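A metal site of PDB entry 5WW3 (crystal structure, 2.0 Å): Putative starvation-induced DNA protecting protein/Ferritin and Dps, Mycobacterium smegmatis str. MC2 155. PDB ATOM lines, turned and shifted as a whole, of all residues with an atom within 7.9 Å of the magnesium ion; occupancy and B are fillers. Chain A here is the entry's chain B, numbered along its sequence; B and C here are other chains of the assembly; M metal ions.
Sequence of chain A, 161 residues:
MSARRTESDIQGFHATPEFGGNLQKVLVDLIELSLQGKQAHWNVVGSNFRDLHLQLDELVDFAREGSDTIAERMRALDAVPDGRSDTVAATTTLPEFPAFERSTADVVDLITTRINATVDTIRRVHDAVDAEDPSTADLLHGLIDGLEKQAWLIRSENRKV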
ATOM      1  N   SER A  47     -32.259  11.752   7.994  1.00  0.00           N
ATOM      2  CA  SER A  47     -31.822  10.912   6.885  1.00  0.00           C
ATOM      3  C   SER A  47     -30.367  10.463   7.046  1.00  0.00           C
ATOM      4  O   SER A  47     -29.454  11.288   7.140  1.00  0.00           O
ATOM      5  CB  SER A  47     -32.029  11.646   5.561  1.00  0.00           C
ATOM      6  OG  SER A  47     -33.373  12.070   5.431  1.00  0.00           O
ATOM      7  N   ASN A  48     -30.163   9.143   7.092  1.00  0.00           N
ATOM      8  CA  ASN A  48     -28.853   8.502   7.291  1.00  0.00           C
ATOM      9  C   ASN A  48     -28.257   8.761   8.676  1.00  0.00           C
ATOM     10  O   ASN A  48     -27.036   8.858   8.844  1.00  0.00           O
ATOM     11  CB  ASN A  48     -27.864   8.859   6.174  1.00  0.00           C
ATOM     12  CG  ASN A  48     -26.771   7.835   6.013  1.00  0.00           C
ATOM     13  OD1 ASN A  48     -26.979   6.646   6.306  1.00  0.00           O
ATOM     14  ND2 ASN A  48     -25.606   8.263   5.542  1.00  0.00           N
ATOM     15  N   PHE A  49     -29.153   8.872   9.657  1.00  0.00           N
ATOM     16  CA  PHE A  49     -28.810   8.935  11.062  1.00  0.00           C
ATOM     17  C   PHE A  49     -27.702   7.941  11.440  1.00  0.00           C
ATOM     18  O   PHE A  49     -26.665   8.335  11.980  1.00  0.00           O
ATOM     19  CB  PHE A  49     -30.050   8.665  11.930  1.00  0.00           C
ATOM     20  CG  PHE A  49     -29.730   8.281  13.345  1.00  0.00           C
ATOM     21  CD1 PHE A  49     -29.286   9.254  14.258  1.00  0.00           C
ATOM     22  CD2 PHE A  49     -29.860   6.963  13.774  1.00  0.00           C
ATOM     23  CE1 PHE A  49     -28.983   8.903  15.572  1.00  0.00           C
ATOM     24  CE2 PHE A  49     -29.538   6.604  15.083  1.00  0.00           C
ATOM     25  CZ  PHE A  49     -29.110   7.579  15.978  1.00  0.00           C
ATOM     26  N   ARG A  50     -27.933   6.667  11.129  1.00  0.00           N
ATOM     27  CA  ARG A  50     -27.146   5.586  11.718  1.00  0.00           C
ATOM     28  C   ARG A  50     -25.672   5.658  11.303  1.00  0.00           C
ATOM     29  O   ARG A  50     -24.785   5.601  12.179  1.00  0.00           O
ATOM     30  CB  ARG A  50     -27.769   4.223  11.415  1.00  0.00           C
ATOM     31  CG  ARG A  50     -27.067   3.068  12.119  1.00  0.00           C
ATOM     32  CD  ARG A  50     -27.737   1.746  11.791  1.00  0.00           C
ATOM     33  NE  ARG A  50     -27.049   0.620  12.410  1.00  0.00           N
ATOM     34  CZ  ARG A  50     -26.050  -0.075  11.861  1.00  0.00           C
ATOM     35  NH1 ARG A  50     -25.566   0.259  10.658  1.00  0.00           N
ATOM     36  NH2 ARG A  50     -25.504  -1.090  12.528  1.00  0.00           N
ATOM     37  N   ASP A  51     -25.423   5.786  10.003  1.00  0.00           N
ATOM     38  CA  ASP A  51     -24.071   5.994   9.484  1.00  0.00           C
ATOM     39  C   ASP A  51     -23.334   7.129  10.182  1.00  0.00           C
ATOM     40  O   ASP A  51     -22.167   6.971  10.517  1.00  0.00           O
ATOM     41  CB  ASP A  51     -24.098   6.282   7.981  1.00  0.00           C
ATOM     42  CG  ASP A  51     -23.938   5.038   7.134  1.00  0.00           C
ATOM     43  OD1 ASP A  51     -23.202   4.107   7.533  1.00  0.00           O
ATOM     44  OD2 ASP A  51     -24.548   4.986   6.058  1.00  0.00           O
ATOM     45  N   LEU A  52     -24.022   8.248  10.401  1.00  0.00           N
ATOM     46  CA  LEU A  52     -23.390   9.408  11.051  1.00  0.00           C
ATOM     47  C   LEU A  52     -23.126   9.174  12.522  1.00  0.00           C
ATOM     48  O   LEU A  52     -22.030   9.459  12.992  1.00  0.00           O
ATOM     49  CB  LEU A  52     -24.200  10.701  10.848  1.00  0.00           C
ATOM     50  CG  LEU A  52     -23.764  11.624   9.693  1.00  0.00           C
ATOM     51  CD1 LEU A  52     -22.324  12.103   9.849  1.00  0.00           C
ATOM     52  CD2 LEU A  52     -23.999  10.979   8.318  1.00  0.00           C
ATOM     53  N   GLU A 157     -20.958  12.616   2.552  1.00  0.00           N
ATOM     54  CA  GLU A 157     -22.425  12.572   2.690  1.00  0.00           C
ATOM     55  C   GLU A 157     -23.159  13.759   2.021  1.00  0.00           C
ATOM     56  O   GLU A 157     -24.230  13.569   1.429  1.00  0.00           O
ATOM     57  CB  GLU A 157     -22.810  12.445   4.165  1.00  0.00           C
ATOM     58  CG  GLU A 157     -24.306  12.602   4.494  1.00  0.00           C
ATOM     59  CD  GLU A 157     -25.183  11.455   4.020  1.00  0.00           C
ATOM     60  OE1 GLU A 157     -26.395  11.674   3.864  1.00  0.00           O
ATOM     61  OE2 GLU A 157     -24.687  10.328   3.806  1.00  0.00           O
ATOM     62  N   SER B  47     -25.464  11.249  -0.783  1.00  0.00           N
ATOM     63  CA  SER B  47     -26.421  10.655   0.163  1.00  0.00           C
ATOM     64  C   SER B  47     -26.159   9.186   0.420  1.00  0.00           C
ATOM     65  O   SER B  47     -26.099   8.395  -0.515  1.00  0.00           O
ATOM     66  CB  SER B  47     -27.853  10.847  -0.358  1.00  0.00           C
ATOM     67  OG  SER B  47     -28.173  12.213  -0.407  1.00  0.00           O
ATOM     68  N   ASN B  48     -26.001   8.837   1.695  1.00  0.00           N
ATOM     69  CA  ASN B  48     -25.672   7.469   2.151  1.00  0.00           C
ATOM     70  C   ASN B  48     -24.299   6.952   1.679  1.00  0.00           C
ATOM     71  O   ASN B  48     -24.122   5.758   1.421  1.00  0.00           O
ATOM     72  CB  ASN B  48     -26.807   6.463   1.822  1.00  0.00           C
ATOM     73  CG  ASN B  48     -26.803   5.265   2.762  1.00  0.00           C
ATOM     74  OD1 ASN B  48     -26.316   5.364   3.889  1.00  0.00           O
ATOM     75  ND2 ASN B  48     -27.331   4.136   2.308  1.00  0.00           N
ATOM     76  N   PHE B  49     -23.333   7.880   1.582  1.00  0.00           N
ATOM     77  CA  PHE B  49     -21.950   7.583   1.217  1.00  0.00           C
ATOM     78  C   PHE B  49     -21.365   6.404   2.012  1.00  0.00           C
ATOM     79  O   PHE B  49     -20.824   5.478   1.411  1.00  0.00           O
ATOM     80  CB  PHE B  49     -21.044   8.814   1.446  1.00  0.00           C
ATOM     81  CG  PHE B  49     -19.571   8.486   1.538  1.00  0.00           C
ATOM     82  CD1 PHE B  49     -18.929   8.407   2.790  1.00  0.00           C
ATOM     83  CD2 PHE B  49     -18.814   8.238   0.393  1.00  0.00           C
ATOM     84  CE1 PHE B  49     -17.563   8.089   2.883  1.00  0.00           C
ATOM     85  CE2 PHE B  49     -17.451   7.924   0.473  1.00  0.00           C
ATOM     86  CZ  PHE B  49     -16.840   7.851   1.725  1.00  0.00           C
ATOM     87  N   ARG B  50     -21.485   6.464   3.335  1.00  0.00           N
ATOM     88  CA  ARG B  50     -20.785   5.532   4.217  1.00  0.00           C
ATOM     89  C   ARG B  50     -21.213   4.078   4.016  1.00  0.00           C
ATOM     90  O   ARG B  50     -20.358   3.209   3.866  1.00  0.00           O
ATOM     91  CB  ARG B  50     -20.902   5.951   5.698  1.00  0.00           C
ATOM     92  CG  ARG B  50     -20.082   5.115   6.662  1.00  0.00           C
ATOM     93  CD  ARG B  50     -20.157   5.649   8.091  1.00  0.00           C
ATOM     94  NE  ARG B  50     -19.402   4.829   9.042  1.00  0.00           N
ATOM     95  CZ  ARG B  50     -19.882   3.750   9.660  1.00  0.00           C
ATOM     96  NH1 ARG B  50     -21.115   3.325   9.410  1.00  0.00           N
ATOM     97  NH2 ARG B  50     -19.111   3.074  10.504  1.00  0.00           N
ATOM     98  N   ASP B  51     -22.532   3.841   4.009  1.00  0.00           N
ATOM     99  CA  ASP B  51     -23.082   2.506   3.766  1.00  0.00           C
ATOM    100  C   ASP B  51     -22.532   1.912   2.476  1.00  0.00           C
ATOM    101  O   ASP B  51     -22.114   0.758   2.448  1.00  0.00           O
ATOM    102  CB  ASP B  51     -24.602   2.536   3.696  1.00  0.00           C
ATOM    103  CG  ASP B  51     -25.268   2.195   5.014  1.00  0.00           C
ATOM    104  OD1 ASP B  51     -24.762   1.328   5.756  1.00  0.00           O
ATOM    105  OD2 ASP B  51     -26.330   2.790   5.297  1.00  0.00           O
ATOM    106  N   LEU B  52     -22.527   2.725   1.413  1.00  0.00           N
ATOM    107  CA  LEU B  52     -22.034   2.279   0.105  1.00  0.00           C
ATOM    108  C   LEU B  52     -20.530   2.072   0.096  1.00  0.00           C
ATOM    109  O   LEU B  52     -20.060   1.048  -0.383  1.00  0.00           O
ATOM    110  CB  LEU B  52     -22.486   3.246  -1.008  1.00  0.00           C
ATOM    111  CG  LEU B  52     -23.775   2.894  -1.771  1.00  0.00           C
ATOM    112  CD1 LEU B  52     -23.658   1.530  -2.447  1.00  0.00           C
ATOM    113  CD2 LEU B  52     -24.997   2.970  -0.862  1.00  0.00           C
ATOM    114  N   GLU B 157     -30.758   0.053  -2.227  1.00  0.00           N
ATOM    115  CA  GLU B 157     -30.631   1.514  -1.996  1.00  0.00           C
ATOM    116  C   GLU B 157     -31.467   2.365  -2.961  1.00  0.00           C
ATOM    117  O   GLU B 157     -32.053   3.364  -2.533  1.00  0.00           O
ATOM    118  CB  GLU B 157     -29.148   1.910  -2.070  1.00  0.00           C
ATOM    119  CG  GLU B 157     -28.852   3.416  -2.009  1.00  0.00           C
ATOM    120  CD  GLU B 157     -29.288   4.099  -0.718  1.00  0.00           C
ATOM    121  OE1 GLU B 157     -29.224   3.508   0.381  1.00  0.00           O
ATOM    122  OE2 GLU B 157     -29.686   5.270  -0.801  1.00  0.00           O
ATOM    123  N   SER C  47     -34.010   4.164   0.188  1.00  0.00           N
ATOM    124  CA  SER C  47     -32.995   5.080   0.724  1.00  0.00           C
ATOM    125  C   SER C  47     -32.516   4.623   2.096  1.00  0.00           C
ATOM    126  O   SER C  47     -33.321   4.430   3.004  1.00  0.00           O
ATOM    127  CB  SER C  47     -33.535   6.503   0.799  1.00  0.00           C
ATOM    128  OG  SER C  47     -32.527   7.409   1.178  1.00  0.00           O
ATOM    129  N   ASN C  48     -31.209   4.459   2.233  1.00  0.00           N
ATOM    130  CA  ASN C  48     -30.573   4.015   3.474  1.00  0.00           C
ATOM    131  C   ASN C  48     -30.962   2.598   3.884  1.00  0.00           C
ATOM    132  O   ASN C  48     -31.005   2.274   5.087  1.00  0.00           O
ATOM    133  CB  ASN C  48     -30.773   5.022   4.625  1.00  0.00           C
ATOM    134  CG  ASN C  48     -29.678   4.922   5.657  1.00  0.00           C
ATOM    135  OD1 ASN C  48     -28.554   4.553   5.309  1.00  0.00           O
ATOM    136  ND2 ASN C  48     -29.988   5.222   6.915  1.00  0.00           N
ATOM    137  N   PHE C  49     -31.213   1.748   2.884  1.00  0.00           N
ATOM    138  CA  PHE C  49     -31.473   0.318   3.065  1.00  0.00           C
ATOM    139  C   PHE C  49     -30.463  -0.343   4.015  1.00  0.00           C
ATOM    140  O   PHE C  49     -30.863  -1.004   4.970  1.00  0.00           O
ATOM    141  CB  PHE C  49     -31.472  -0.422   1.710  1.00  0.00           C
ATOM    142  CG  PHE C  49     -31.242  -1.901   1.836  1.00  0.00           C
ATOM    143  CD1 PHE C  49     -32.285  -2.743   2.193  1.00  0.00           C
ATOM    144  CD2 PHE C  49     -29.960  -2.444   1.620  1.00  0.00           C
ATOM    145  CE1 PHE C  49     -32.064  -4.119   2.340  1.00  0.00           C
ATOM    146  CE2 PHE C  49     -29.741  -3.804   1.772  1.00  0.00           C
ATOM    147  CZ  PHE C  49     -30.793  -4.642   2.132  1.00  0.00           C
ATOM    148  N   ARG C  50     -29.171  -0.187   3.739  1.00  0.00           N
ATOM    149  CA  ARG C  50     -28.137  -0.958   4.434  1.00  0.00           C
ATOM    150  C   ARG C  50     -28.165  -0.725   5.939  1.00  0.00           C
ATOM    151  O   ARG C  50     -28.197  -1.698   6.714  1.00  0.00           O
ATOM    152  CB  ARG C  50     -26.743  -0.722   3.824  1.00  0.00           C
ATOM    153  CG  ARG C  50     -25.665  -1.626   4.395  1.00  0.00           C
ATOM    154  CD  ARG C  50     -24.324  -1.361   3.758  1.00  0.00           C
ATOM    155  NE  ARG C  50     -23.271  -2.213   4.324  1.00  0.00           N
ATOM    156  CZ  ARG C  50     -22.524  -1.900   5.389  1.00  0.00           C
ATOM    157  NH1 ARG C  50     -22.709  -0.759   6.029  1.00  0.00           N
ATOM    158  NH2 ARG C  50     -21.599  -2.740   5.812  1.00  0.00           N
ATOM    159  N   ASP C  51     -28.175   0.538   6.361  1.00  0.00           N
ATOM    160  CA  ASP C  51     -28.293   0.888   7.781  1.00  0.00           C
ATOM    161  C   ASP C  51     -29.465   0.231   8.470  1.00  0.00           C
ATOM    162  O   ASP C  51     -29.302  -0.312   9.576  1.00  0.00           O
ATOM    163  CB  ASP C  51     -28.402   2.399   7.981  1.00  0.00           C
ATOM    164  CG  ASP C  51     -27.061   3.056   8.239  1.00  0.00           C
ATOM    165  OD1 ASP C  51     -26.208   2.470   8.934  1.00  0.00           O
ATOM    166  OD2 ASP C  51     -26.866   4.175   7.738  1.00  0.00           O
ATOM    167  N   LEU C  52     -30.636   0.267   7.836  1.00  0.00           N
ATOM    168  CA  LEU C  52     -31.845  -0.289   8.447  1.00  0.00           C
ATOM    169  C   LEU C  52     -31.807  -1.804   8.467  1.00  0.00           C
ATOM    170  O   LEU C  52     -32.176  -2.393   9.465  1.00  0.00           O
ATOM    171  CB  LEU C  52     -33.136   0.251   7.810  1.00  0.00           C
ATOM    172  CG  LEU C  52     -33.767   1.501   8.459  1.00  0.00           C
ATOM    173  CD1 LEU C  52     -34.207   1.218   9.890  1.00  0.00           C
ATOM    174  CD2 LEU C  52     -32.843   2.730   8.410  1.00  0.00           C
ATOM    175  N   GLU C 157     -33.961   8.026  12.009  1.00  0.00           N
ATOM    176  CA  GLU C 157     -33.909   8.099  10.540  1.00  0.00           C
ATOM    177  C   GLU C 157     -35.013   9.001   9.959  1.00  0.00           C
ATOM    178  O   GLU C 157     -34.746   9.757   9.032  1.00  0.00           O
ATOM    179  CB  GLU C 157     -33.991   6.677   9.954  1.00  0.00           C
ATOM    180  CG  GLU C 157     -34.187   6.557   8.439  1.00  0.00           C
ATOM    181  CD  GLU C 157     -33.031   7.111   7.615  1.00  0.00           C
ATOM    182  OE1 GLU C 157     -33.301   7.573   6.486  1.00  0.00           O
ATOM    183  OE2 GLU C 157     -31.873   7.096   8.063  1.00  0.00           O
HETATM  184 MG    MG M   1     -26.617   4.769   5.726  1.00  0.00          MG
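The side-chain amide nitrogen (ND2) of Asn 48 of chain A lies within hydrogen-bond range of the side-chain carboxylate (OE2) of Glu 157 of chain A, at 2.8 Å.
The side-chain carboxylate of Asp 51 of chain A lies within salt-bridge range of the guanidinium group of Arg 50 of chain B (2.9 Å).
The side-chain amide nitrogen of Asn 48 of chain C lies within hydrogen-bond range of the side-chain carboxylate of Glu 157 of chain C, at 2.9 Å.
NH1 of Arg 50 of chain C is in salt-bridge range of OD1 of Asp 51 of chain B, 2.9 Å away.
The side-chain carboxylate (OE1) of Glu 157 of chain B lies within hydrogen-bond range of the side-chain amide nitrogen (ND2) of Asn 48 of chain B (2.8 Å).
The backbone NH (N) of Asn 48 of chain C sits at hydrogen-bond distance from the side-chain carboxylate (OE1) of Glu 157 of chain B, at 2.9 Å.
The guanidinium group (NH1) of Arg 50 of chain A is in salt-bridge range of the side-chain carboxylate (OD1) of Asp 51 of chain C (2.9 Å).
The backbone NH of Asn 48 of chain A sits at hydrogen-bond distance from the side-chain carboxylate of Glu 157 of chain C (2.8 Å).
The magnesium ion is bound by OD1 of Asn 48 of chain B, 2.0 Å away.
The side-chain amide oxygen (OD1) of Asn 48 of chain C is bound to the magnesium ion.
OD1 of Asn 48 of chain A is bound to the magnesium ion (2.0 Å).
The magnesium ion is bound by OD2 of Asp 51 of chain B (2.0 Å).
The magnesium ion is bound by OD2 of Asp 51 of chain A.
OD2 of Asp 51 of chain C is bound to the magnesium ion (2.1 Å).
The magnesium ion has six donor atoms within binding distance.
Within 4 Å of the magnesium ion: Asn 48 of chain A, Asp 51 of chain A, Asn 48 of chain B, Asp 51 of chain B, Asn 48 of chain C and Asp 51 of chain C.
The nearest printed residue that does not touch the magnesium ion is Arg 50 of chain B (5.7 Å).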
